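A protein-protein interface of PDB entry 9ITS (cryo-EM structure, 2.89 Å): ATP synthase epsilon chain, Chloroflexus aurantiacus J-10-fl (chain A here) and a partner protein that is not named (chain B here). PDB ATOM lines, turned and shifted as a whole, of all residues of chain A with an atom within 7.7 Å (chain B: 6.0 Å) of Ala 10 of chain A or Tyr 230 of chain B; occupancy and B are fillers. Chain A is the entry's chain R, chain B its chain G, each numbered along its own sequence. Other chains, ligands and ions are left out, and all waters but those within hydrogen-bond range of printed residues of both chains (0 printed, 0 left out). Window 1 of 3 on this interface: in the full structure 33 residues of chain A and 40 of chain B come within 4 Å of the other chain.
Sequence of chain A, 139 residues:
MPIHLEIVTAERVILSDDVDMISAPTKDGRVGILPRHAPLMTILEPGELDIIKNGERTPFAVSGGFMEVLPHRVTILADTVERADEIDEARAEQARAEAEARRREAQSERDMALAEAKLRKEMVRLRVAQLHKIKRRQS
Printed residues of chain B that touch a printed residue of chain A: Ala 41, Thr 42, Tyr 45, Lys 148, Leu 149, Arg 223 and Tyr 230.
Hydrophobic or aromatic side chains of chain B that line the printed part of chain A: Ala 41, Tyr 45, Leu 149 and Tyr 230.
Hydrophobic or aromatic side chains of chain A that line the printed part of chain B: Ala 10 and Leu 77.
Among the printed residues, Asp or Glu carboxylates within 4 Å of a Lys or Arg side-chain nitrogen of the other chain: Asp 79 of chain A with Arg 223 of chain B (3.6 Å).
OE2 of Glu 11 of chain A sits at hydrogen-bond distance from N of Leu 149 of chain B, at 3.1 Å.
The guanidinium group (NE) of Arg 223 of chain B lies within salt-bridge range of the side-chain carboxylate (OD1) of Asp 79 of chain A (3.6 Å).
NE of Arg 223 of chain B lies within hydrogen-bond range of OH of Tyr 45 of chain B (3.3 Å).
NH1 of Arg 223 of chain B lies within salt-bridge range of OE1 of Glu 226 of chain B, 3.8 Å away.
The backbone NH (N) of Val 8 of chain A sits at hydrogen-bond distance from the backbone carbonyl oxygen (O) of Ile 76 of chain A, 3.1 Å away.
The backbone NH of Ala 78 of chain A sits at hydrogen-bond distance from the backbone carbonyl oxygen of Val 8 of chain A, 3.5 Å away.
Val 8 of chain A touches Tyr 45 of chain B.
Thr 9 of chain A touches Tyr 45 of chain B (O to CB, 3.3 Å).
O of Ala 10 of chain A touches CG2 of Thr 42 of chain B, at 3.2 Å.
Tyr 45 of chain B touches Ala 10 of chain A.
CD1 of Leu 149 of chain B touches CB of Ala 10 of chain A (3.7 Å).
Tyr 230 of chain B touches Ala 10 of chain A.
O of Glu 11 of chain A touches CB of Ala 41 of chain B, at 3.9 Å.
OG1 of Thr 42 of chain B touches O of Glu 11 of chain A, 3.8 Å away.
OE2 of Glu 11 of chain A touches CB of Lys 148 of chain B, at 3.4 Å.
CD2 of Leu 77 of chain A touches CD1 of Tyr 45 of chain B, 3.5 Å away.
Ala 10 of chain A touches just these residues of chain B: Thr 42 (3.2 Å), Tyr 45 (3.5 Å), Leu 149 (3.7 Å) and Tyr 230 (3.6 Å).
Of chain A, only Ala 10 (3.6 Å) and Glu 11 (3.7 Å) come within 4 Å of Tyr 230 of chain B.
Of the printed residues of chain A, Tyr 45 of chain B touches Val 8 (3.6 Å), Thr 9 (3.3 Å), Ala 10 (3.5 Å) and Leu 77 (3.5 Å).
Of the printed residues of chain A, Lys 148 of chain B touches Glu 11.
Of the printed residues of chain A, Leu 149 of chain B touches Ala 10 and Glu 11.
Ile 76 of chain A touches none of the printed residues of chain B.
Ala 232 of chain B touches none of the printed residues of chain A.
The nearest residue of chain B that does not touch Ala 10 of chain A is Arg 223 of chain B (4.3 Å).
The nearest residue of chain A that does not touch Tyr 230 of chain B is Arg 12 of chain A (7.1 Å).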
ATOM      1  N   VAL A   8     -13.137 -11.996  21.259  1.00  0.00           N
ATOM      2  CA  VAL A   8     -13.425 -10.692  20.679  1.00  0.00           C
ATOM      3  C   VAL A   8     -14.856 -10.310  21.033  1.00  0.00           C
ATOM      4  O   VAL A   8     -15.763 -11.148  20.973  1.00  0.00           O
ATOM      5  CB  VAL A   8     -13.209 -10.687  19.155  1.00  0.00           C
ATOM      6  CG1 VAL A   8     -11.732 -10.775  18.834  1.00  0.00           C
ATOM      7  CG2 VAL A   8     -13.936 -11.847  18.508  1.00  0.00           C
ATOM      8  N   THR A   9     -15.048  -9.056  21.421  1.00  0.00           N
ATOM      9  CA  THR A   9     -16.357  -8.508  21.733  1.00  0.00           C
ATOM     10  C   THR A   9     -16.736  -7.515  20.641  1.00  0.00           C
ATOM     11  O   THR A   9     -15.887  -7.066  19.865  1.00  0.00           O
ATOM     12  CB  THR A   9     -16.345  -7.837  23.115  1.00  0.00           C
ATOM     13  OG1 THR A   9     -15.660  -8.687  24.041  1.00  0.00           O
ATOM     14  CG2 THR A   9     -17.757  -7.633  23.649  1.00  0.00           C
ATOM     15  N   ALA A  10     -18.030  -7.187  20.570  1.00  0.00           N
ATOM     16  CA  ALA A  10     -18.523  -6.274  19.546  1.00  0.00           C
ATOM     17  C   ALA A  10     -17.885  -4.895  19.627  1.00  0.00           C
ATOM     18  O   ALA A  10     -17.862  -4.179  18.621  1.00  0.00           O
ATOM     19  CB  ALA A  10     -20.042  -6.148  19.651  1.00  0.00           C
ATOM     20  N   GLU A  11     -17.369  -4.505  20.789  1.00  0.00           N
ATOM     21  CA  GLU A  11     -16.707  -3.217  20.947  1.00  0.00           C
ATOM     22  C   GLU A  11     -15.195  -3.295  20.796  1.00  0.00           C
ATOM     23  O   GLU A  11     -14.592  -2.397  20.203  1.00  0.00           O
ATOM     24  CB  GLU A  11     -17.048  -2.609  22.311  1.00  0.00           C
ATOM     25  CG  GLU A  11     -18.426  -1.972  22.379  1.00  0.00           C
ATOM     26  CD  GLU A  11     -19.510  -2.962  22.753  1.00  0.00           C
ATOM     27  OE1 GLU A  11     -19.184  -4.145  22.988  1.00  0.00           O
ATOM     28  OE2 GLU A  11     -20.689  -2.557  22.813  1.00  0.00           O
ATOM     29  N   ARG A  12     -14.564  -4.348  21.313  1.00  0.00           N
ATOM     30  CA  ARG A  12     -13.110  -4.423  21.304  1.00  0.00           C
ATOM     31  C   ARG A  12     -12.672  -5.876  21.397  1.00  0.00           C
ATOM     32  O   ARG A  12     -13.433  -6.750  21.818  1.00  0.00           O
ATOM     33  CB  ARG A  12     -12.506  -3.612  22.455  1.00  0.00           C
ATOM     34  CG  ARG A  12     -13.009  -4.029  23.827  1.00  0.00           C
ATOM     35  CD  ARG A  12     -12.541  -3.067  24.905  1.00  0.00           C
ATOM     36  NE  ARG A  12     -11.090  -3.063  25.038  1.00  0.00           N
ATOM     37  CZ  ARG A  12     -10.413  -3.837  25.876  1.00  0.00           C
ATOM     38  NH1 ARG A  12     -11.029  -4.688  26.680  1.00  0.00           N
ATOM     39  NH2 ARG A  12      -9.087  -3.755  25.909  1.00  0.00           N
ATOM     40  N   VAL A  13     -11.428  -6.117  20.994  1.00  0.00           N
ATOM     41  CA  VAL A  13     -10.806  -7.427  21.149  1.00  0.00           C
ATOM     42  C   VAL A  13     -10.339  -7.577  22.588  1.00  0.00           C
ATOM     43  O   VAL A  13      -9.662  -6.695  23.128  1.00  0.00           O
ATOM     44  CB  VAL A  13      -9.633  -7.592  20.170  1.00  0.00           C
ATOM     45  CG1 VAL A  13      -8.928  -8.920  20.398  1.00  0.00           C
ATOM     46  CG2 VAL A  13     -10.118  -7.483  18.745  1.00  0.00           C
ATOM     47  N   ILE A  14     -10.696  -8.693  23.215  1.00  0.00           N
ATOM     48  CA  ILE A  14     -10.302  -8.929  24.598  1.00  0.00           C
ATOM     49  C   ILE A  14      -8.984  -9.685  24.681  1.00  0.00           C
ATOM     50  O   ILE A  14      -8.068  -9.279  25.400  1.00  0.00           O
ATOM     51  CB  ILE A  14     -11.417  -9.673  25.354  1.00  0.00           C
ATOM     52  CG1 ILE A  14     -12.722  -8.880  25.301  1.00  0.00           C
ATOM     53  CG2 ILE A  14     -11.004  -9.881  26.791  1.00  0.00           C
ATOM     54  CD1 ILE A  14     -12.651  -7.539  25.986  1.00  0.00           C
ATOM     55  N   ILE A  76     -14.257 -16.667  20.206  1.00  0.00           N
ATOM     56  CA  ILE A  76     -15.441 -16.445  21.028  1.00  0.00           C
ATOM     57  C   ILE A  76     -16.031 -15.094  20.660  1.00  0.00           C
ATOM     58  O   ILE A  76     -15.404 -14.050  20.881  1.00  0.00           O
ATOM     59  CB  ILE A  76     -15.142 -16.524  22.533  1.00  0.00           C
ATOM     60  CG1 ILE A  76     -14.659 -17.923  22.929  1.00  0.00           C
ATOM     61  CG2 ILE A  76     -16.372 -16.144  23.339  1.00  0.00           C
ATOM     62  CD1 ILE A  76     -13.177 -18.130  22.832  1.00  0.00           C
ATOM     63  N   LEU A  77     -17.236 -15.119  20.105  1.00  0.00           N
ATOM     64  CA  LEU A  77     -17.990 -13.917  19.764  1.00  0.00           C
ATOM     65  C   LEU A  77     -18.994 -13.615  20.874  1.00  0.00           C
ATOM     66  O   LEU A  77     -20.173 -13.946  20.787  1.00  0.00           O
ATOM     67  CB  LEU A  77     -18.691 -14.109  18.423  1.00  0.00           C
ATOM     68  CG  LEU A  77     -17.800 -14.283  17.192  1.00  0.00           C
ATOM     69  CD1 LEU A  77     -18.639 -14.622  15.975  1.00  0.00           C
ATOM     70  CD2 LEU A  77     -16.981 -13.041  16.937  1.00  0.00           C
ATOM     71  N   ALA A  78     -18.500 -13.029  21.958  1.00  0.00           N
ATOM     72  CA  ALA A  78     -19.323 -12.874  23.147  1.00  0.00           C
ATOM     73  C   ALA A  78     -20.007 -11.512  23.171  1.00  0.00           C
ATOM     74  O   ALA A  78     -19.504 -10.527  22.626  1.00  0.00           O
ATOM     75  CB  ALA A  78     -18.480 -13.063  24.404  1.00  0.00           C
ATOM     76  N   ASP A  79     -21.171 -11.467  23.822  1.00  0.00           N
ATOM     77  CA  ASP A  79     -21.971 -10.247  23.853  1.00  0.00           C
ATOM     78  C   ASP A  79     -21.371  -9.211  24.799  1.00  0.00           C
ATOM     79  O   ASP A  79     -20.995  -8.113  24.377  1.00  0.00           O
ATOM     80  CB  ASP A  79     -23.410 -10.577  24.257  1.00  0.00           C
ATOM     81  CG  ASP A  79     -24.088 -11.515  23.279  1.00  0.00           C
ATOM     82  OD1 ASP A  79     -23.404 -12.018  22.363  1.00  0.00           O
ATOM     83  OD2 ASP A  79     -25.306 -11.753  23.427  1.00  0.00           O
ATOM     84  N   THR A  80     -21.280  -9.544  26.085  1.00  0.00           N
ATOM     85  CA  THR A  80     -20.643  -8.677  27.068  1.00  0.00           C
ATOM     86  C   THR A  80     -19.867  -9.540  28.052  1.00  0.00           C
ATOM     87  O   THR A  80     -20.346 -10.597  28.471  1.00  0.00           O
ATOM     88  CB  THR A  80     -21.667  -7.791  27.795  1.00  0.00           C
ATOM     89  OG1 THR A  80     -21.010  -7.034  28.820  1.00  0.00           O
ATOM     90  CG2 THR A  80     -22.792  -8.618  28.400  1.00  0.00           C
ATOM     91  N   ALA B  41     -11.345  -1.089  15.728  1.00  0.00           N
ATOM     92  CA  ALA B  41     -11.419  -2.024  16.846  1.00  0.00           C
ATOM     93  C   ALA B  41     -12.634  -2.937  16.723  1.00  0.00           C
ATOM     94  O   ALA B  41     -12.577  -4.111  17.103  1.00  0.00           O
ATOM     95  CB  ALA B  41     -11.453  -1.258  18.168  1.00  0.00           C
ATOM     96  N   THR B  42     -13.743  -2.410  16.200  1.00  0.00           N
ATOM     97  CA  THR B  42     -14.942  -3.219  16.009  1.00  0.00           C
ATOM     98  C   THR B  42     -14.785  -4.186  14.840  1.00  0.00           C
ATOM     99  O   THR B  42     -15.378  -5.270  14.851  1.00  0.00           O
ATOM    100  CB  THR B  42     -16.147  -2.297  15.799  1.00  0.00           C
ATOM    101  OG1 THR B  42     -16.298  -1.446  16.941  1.00  0.00           O
ATOM    102  CG2 THR B  42     -17.434  -3.087  15.596  1.00  0.00           C
ATOM    103  N   TYR B  45     -14.305  -8.207  15.152  1.00  0.00           N
ATOM    104  CA  TYR B  45     -15.503  -8.920  15.584  1.00  0.00           C
ATOM    105  C   TYR B  45     -16.471  -9.111  14.425  1.00  0.00           C
ATOM    106  O   TYR B  45     -17.020 -10.204  14.236  1.00  0.00           O
ATOM    107  CB  TYR B  45     -16.181  -8.163  16.727  1.00  0.00           C
ATOM    108  CG  TYR B  45     -17.491  -8.765  17.193  1.00  0.00           C
ATOM    109  CD1 TYR B  45     -17.515  -9.761  18.158  1.00  0.00           C
ATOM    110  CD2 TYR B  45     -18.705  -8.331  16.672  1.00  0.00           C
ATOM    111  CE1 TYR B  45     -18.707 -10.311  18.588  1.00  0.00           C
ATOM    112  CE2 TYR B  45     -19.900  -8.876  17.097  1.00  0.00           C
ATOM    113  CZ  TYR B  45     -19.895  -9.864  18.054  1.00  0.00           C
ATOM    114  OH  TYR B  45     -21.084 -10.408  18.480  1.00  0.00           O
ATOM    115  N   ALA B 146     -18.936   7.224  20.875  1.00  0.00           N
ATOM    116  CA  ALA B 146     -18.493   5.849  21.100  1.00  0.00           C
ATOM    117  C   ALA B 146     -19.658   5.040  21.652  1.00  0.00           C
ATOM    118  O   ALA B 146     -19.668   4.659  22.829  1.00  0.00           O
ATOM    119  CB  ALA B 146     -17.297   5.809  22.052  1.00  0.00           C
ATOM    120  N   PRO B 147     -20.662   4.757  20.828  1.00  0.00           N
ATOM    121  CA  PRO B 147     -21.829   4.022  21.313  1.00  0.00           C
ATOM    122  C   PRO B 147     -21.538   2.536  21.454  1.00  0.00           C
ATOM    123  O   PRO B 147     -20.658   1.975  20.800  1.00  0.00           O
ATOM    124  CB  PRO B 147     -22.875   4.276  20.226  1.00  0.00           C
ATOM    125  CG  PRO B 147     -22.066   4.380  18.985  1.00  0.00           C
ATOM    126  CD  PRO B 147     -20.739   4.997  19.375  1.00  0.00           C
ATOM    127  N   LYS B 148     -22.302   1.904  22.334  1.00  0.00           N
ATOM    128  CA  LYS B 148     -22.256   0.462  22.514  1.00  0.00           C
ATOM    129  C   LYS B 148     -23.381  -0.189  21.716  1.00  0.00           C
ATOM    130  O   LYS B 148     -24.367   0.451  21.347  1.00  0.00           O
ATOM    131  CB  LYS B 148     -22.364   0.103  23.997  1.00  0.00           C
ATOM    132  CG  LYS B 148     -21.261   0.696  24.853  1.00  0.00           C
ATOM    133  CD  LYS B 148     -21.429   0.317  26.313  1.00  0.00           C
ATOM    134  CE  LYS B 148     -20.347   0.953  27.169  1.00  0.00           C
ATOM    135  NZ  LYS B 148     -18.993   0.443  26.818  1.00  0.00           N
ATOM    136  N   LEU B 149     -23.214  -1.485  21.441  1.00  0.00           N
ATOM    137  CA  LEU B 149     -24.222  -2.208  20.676  1.00  0.00           C
ATOM    138  C   LEU B 149     -25.546  -2.306  21.427  1.00  0.00           C
ATOM    139  O   LEU B 149     -26.599  -2.450  20.795  1.00  0.00           O
ATOM    140  CB  LEU B 149     -23.679  -3.592  20.299  1.00  0.00           C
ATOM    141  CG  LEU B 149     -24.439  -4.508  19.335  1.00  0.00           C
ATOM    142  CD1 LEU B 149     -23.457  -5.393  18.601  1.00  0.00           C
ATOM    143  CD2 LEU B 149     -25.429  -5.387  20.069  1.00  0.00           C
ATOM    144  N   GLU B 150     -25.518  -2.200  22.758  1.00  0.00           N
ATOM    145  CA  GLU B 150     -26.754  -2.162  23.529  1.00  0.00           C
ATOM    146  C   GLU B 150     -27.581  -0.916  23.239  1.00  0.00           C
ATOM    147  O   GLU B 150     -28.799  -0.935  23.450  1.00  0.00           O
ATOM    148  CB  GLU B 150     -26.442  -2.244  25.023  1.00  0.00           C
ATOM    149  CG  GLU B 150     -25.470  -1.185  25.512  1.00  0.00           C
ATOM    150  CD  GLU B 150     -25.215  -1.272  27.002  1.00  0.00           C
ATOM    151  OE1 GLU B 150     -25.629  -2.276  27.619  1.00  0.00           O
ATOM    152  OE2 GLU B 150     -24.600  -0.339  27.558  1.00  0.00           O
ATOM    153  N   ILE B 152     -28.048   0.417  20.184  1.00  0.00           N
ATOM    154  CA  ILE B 152     -28.813   0.103  18.983  1.00  0.00           C
ATOM    155  C   ILE B 152     -29.591  -1.195  19.113  1.00  0.00           C
ATOM    156  O   ILE B 152     -30.330  -1.555  18.182  1.00  0.00           O
ATOM    157  CB  ILE B 152     -27.893   0.014  17.751  1.00  0.00           C
ATOM    158  CG1 ILE B 152     -27.047  -1.256  17.826  1.00  0.00           C
ATOM    159  CG2 ILE B 152     -27.002   1.238  17.665  1.00  0.00           C
ATOM    160  CD1 ILE B 152     -26.689  -1.829  16.487  1.00  0.00           C
ATOM    161  N   ARG B 223     -27.836 -11.579  15.821  1.00  0.00           N
ATOM    162  CA  ARG B 223     -26.557 -10.988  16.202  1.00  0.00           C
ATOM    163  C   ARG B 223     -25.803 -10.466  14.986  1.00  0.00           C
ATOM    164  O   ARG B 223     -25.145  -9.422  15.060  1.00  0.00           O
ATOM    165  CB  ARG B 223     -25.710 -12.002  16.968  1.00  0.00           C
ATOM    166  CG  ARG B 223     -24.605 -11.363  17.789  1.00  0.00           C
ATOM    167  CD  ARG B 223     -25.168 -10.372  18.791  1.00  0.00           C
ATOM    168  NE  ARG B 223     -24.122  -9.758  19.600  1.00  0.00           N
ATOM    169  CZ  ARG B 223     -24.347  -8.976  20.646  1.00  0.00           C
ATOM    170  NH1 ARG B 223     -25.575  -8.689  21.044  1.00  0.00           N
ATOM    171  NH2 ARG B 223     -23.314  -8.466  21.309  1.00  0.00           N
ATOM    172  N   VAL B 225     -27.270  -9.327  12.241  1.00  0.00           N
ATOM    173  CA  VAL B 225     -27.966  -8.092  11.882  1.00  0.00           C
ATOM    174  C   VAL B 225     -27.558  -6.960  12.816  1.00  0.00           C
ATOM    175  O   VAL B 225     -27.319  -5.825  12.379  1.00  0.00           O
ATOM    176  CB  VAL B 225     -29.490  -8.312  11.891  1.00  0.00           C
ATOM    177  CG1 VAL B 225     -30.215  -7.008  11.611  1.00  0.00           C
ATOM    178  CG2 VAL B 225     -29.881  -9.358  10.871  1.00  0.00           C
ATOM    179  N   GLU B 226     -27.467  -7.252  14.115  1.00  0.00           N
ATOM    180  CA  GLU B 226     -27.099  -6.237  15.094  1.00  0.00           C
ATOM    181  C   GLU B 226     -25.692  -5.710  14.847  1.00  0.00           C
ATOM    182  O   GLU B 226     -25.457  -4.501  14.923  1.00  0.00           O
ATOM    183  CB  GLU B 226     -27.217  -6.807  16.506  1.00  0.00           C
ATOM    184  CG  GLU B 226     -28.628  -6.790  17.062  1.00  0.00           C
ATOM    185  CD  GLU B 226     -28.949  -8.018  17.889  1.00  0.00           C
ATOM    186  OE1 GLU B 226     -28.019  -8.793  18.192  1.00  0.00           O
ATOM    187  OE2 GLU B 226     -30.133  -8.208  18.236  1.00  0.00           O
ATOM    188  N   THR B 227     -24.743  -6.598  14.542  1.00  0.00           N
ATOM    189  CA  THR B 227     -23.382  -6.129  14.310  1.00  0.00           C
ATOM    190  C   THR B 227     -23.261  -5.401  12.975  1.00  0.00           C
ATOM    191  O   THR B 227     -22.454  -4.474  12.857  1.00  0.00           O
ATOM    192  CB  THR B 227     -22.383  -7.289  14.412  1.00  0.00           C
ATOM    193  OG1 THR B 227     -21.057  -6.764  14.550  1.00  0.00           O
ATOM    194  CG2 THR B 227     -22.431  -8.192  13.193  1.00  0.00           C
ATOM    195  N   GLN B 228     -24.075  -5.766  11.978  1.00  0.00           N
ATOM    196  CA  GLN B 228     -24.099  -4.993  10.739  1.00  0.00           C
ATOM    197  C   GLN B 228     -24.614  -3.580  10.984  1.00  0.00           C
ATOM    198  O   GLN B 228     -24.031  -2.602  10.492  1.00  0.00           O
ATOM    199  CB  GLN B 228     -24.958  -5.703   9.695  1.00  0.00           C
ATOM    200  CG  GLN B 228     -24.290  -6.890   9.028  1.00  0.00           C
ATOM    201  CD  GLN B 228     -23.285  -6.474   7.976  1.00  0.00           C
ATOM    202  OE1 GLN B 228     -23.559  -5.603   7.150  1.00  0.00           O
ATOM    203  NE2 GLN B 228     -22.113  -7.097   7.998  1.00  0.00           N
ATOM    204  N   ILE B 229     -25.695  -3.452  11.758  1.00  0.00           N
ATOM    205  CA  ILE B 229     -26.230  -2.130  12.078  1.00  0.00           C
ATOM    206  C   ILE B 229     -25.223  -1.335  12.901  1.00  0.00           C
ATOM    207  O   ILE B 229     -25.052  -0.128  12.698  1.00  0.00           O
ATOM    208  CB  ILE B 229     -27.583  -2.256  12.802  1.00  0.00           C
ATOM    209  CG1 ILE B 229     -28.621  -2.907  11.892  1.00  0.00           C
ATOM    210  CG2 ILE B 229     -28.089  -0.894  13.239  1.00  0.00           C
ATOM    211  CD1 ILE B 229     -29.803  -3.475  12.636  1.00  0.00           C
ATOM    212  N   TYR B 230     -24.539  -1.996  13.837  1.00  0.00           N
ATOM    213  CA  TYR B 230     -23.536  -1.322  14.655  1.00  0.00           C
ATOM    214  C   TYR B 230     -22.379  -0.809  13.809  1.00  0.00           C
ATOM    215  O   TYR B 230     -21.906   0.319  14.004  1.00  0.00           O
ATOM    216  CB  TYR B 230     -23.030  -2.277  15.733  1.00  0.00           C
ATOM    217  CG  TYR B 230     -22.184  -1.629  16.800  1.00  0.00           C
ATOM    218  CD1 TYR B 230     -22.696  -0.621  17.603  1.00  0.00           C
ATOM    219  CD2 TYR B 230     -20.874  -2.032  17.010  1.00  0.00           C
ATOM    220  CE1 TYR B 230     -21.925  -0.031  18.582  1.00  0.00           C
ATOM    221  CE2 TYR B 230     -20.096  -1.448  17.985  1.00  0.00           C
ATOM    222  CZ  TYR B 230     -20.626  -0.448  18.769  1.00  0.00           C
ATOM    223  OH  TYR B 230     -19.852   0.136  19.742  1.00  0.00           O
ATOM    224  N   GLN B 231     -21.907  -1.624  12.864  1.00  0.00           N
ATOM    225  CA  GLN B 231     -20.841  -1.187  11.971  1.00  0.00           C
ATOM    226  C   GLN B 231     -21.293  -0.011  11.116  1.00  0.00           C
ATOM    227  O   GLN B 231     -20.530   0.938  10.897  1.00  0.00           O
ATOM    228  CB  GLN B 231     -20.383  -2.352  11.096  1.00  0.00           C
ATOM    229  CG  GLN B 231     -19.085  -2.104  10.353  1.00  0.00           C
ATOM    230  CD  GLN B 231     -18.527  -3.366   9.728  1.00  0.00           C
ATOM    231  OE1 GLN B 231     -19.108  -4.443   9.853  1.00  0.00           O
ATOM    232  NE2 GLN B 231     -17.392  -3.240   9.052  1.00  0.00           N
ATOM    233  N   ALA B 232     -22.539  -0.052  10.634  1.00  0.00           N
ATOM    234  CA  ALA B 232     -23.066   1.067   9.858  1.00  0.00           C
ATOM    235  C   ALA B 232     -23.143   2.340  10.695  1.00  0.00           C
ATOM    236  O   ALA B 232     -22.819   3.427  10.210  1.00  0.00           O
ATOM    237  CB  ALA B 232     -24.439   0.714   9.293  1.00  0.00           C
ATOM    238  N   VAL B 233     -23.570   2.223  11.955  1.00  0.00           N
ATOM    239  CA  VAL B 233     -23.659   3.389  12.830  1.00  0.00           C
ATOM    240  C   VAL B 233     -22.278   3.972  13.100  1.00  0.00           C
ATOM    241  O   VAL B 233     -22.096   5.196  13.097  1.00  0.00           O
ATOM    242  CB  VAL B 233     -24.390   3.028  14.136  1.00  0.00           C
ATOM    243  CG1 VAL B 233     -24.321   4.177  15.121  1.00  0.00           C
ATOM    244  CG2 VAL B 233     -25.841   2.703  13.850  1.00  0.00           C
ATOM    245  N   LEU B 234     -21.285   3.116  13.346  1.00  0.00           N
ATOM    246  CA  LEU B 234     -19.930   3.614  13.580  1.00  0.00           C
ATOM    247  C   LEU B 234     -19.361   4.289  12.336  1.00  0.00           C
ATOM    248  O   LEU B 234     -18.708   5.340  12.431  1.00  0.00           O
ATOM    249  CB  LEU B 234     -19.026   2.476  14.043  1.00  0.00           C
ATOM    250  CG  LEU B 234     -19.384   1.871  15.400  1.00  0.00           C
ATOM    251  CD1 LEU B 234     -18.323   0.882  15.835  1.00  0.00           C
ATOM    252  CD2 LEU B 234     -19.563   2.959  16.444  1.00  0.00           C
ATOM    253  N   GLU B 235     -19.603   3.704  11.159  1.00  0.00           N
ATOM    254  CA  GLU B 235     -19.179   4.336   9.915  1.00  0.00           C
ATOM    255  C   GLU B 235     -19.856   5.687   9.729  1.00  0.00           C
ATOM    256  O   GLU B 235     -19.222   6.658   9.297  1.00  0.00           O
ATOM    257  CB  GLU B 235     -19.487   3.417   8.734  1.00  0.00           C
ATOM    258  CG  GLU B 235     -18.768   3.781   7.450  1.00  0.00           C
ATOM    259  CD  GLU B 235     -17.406   3.131   7.347  1.00  0.00           C
ATOM    260  OE1 GLU B 235     -17.086   2.283   8.205  1.00  0.00           O
ATOM    261  OE2 GLU B 235     -16.657   3.461   6.404  1.00  0.00           O
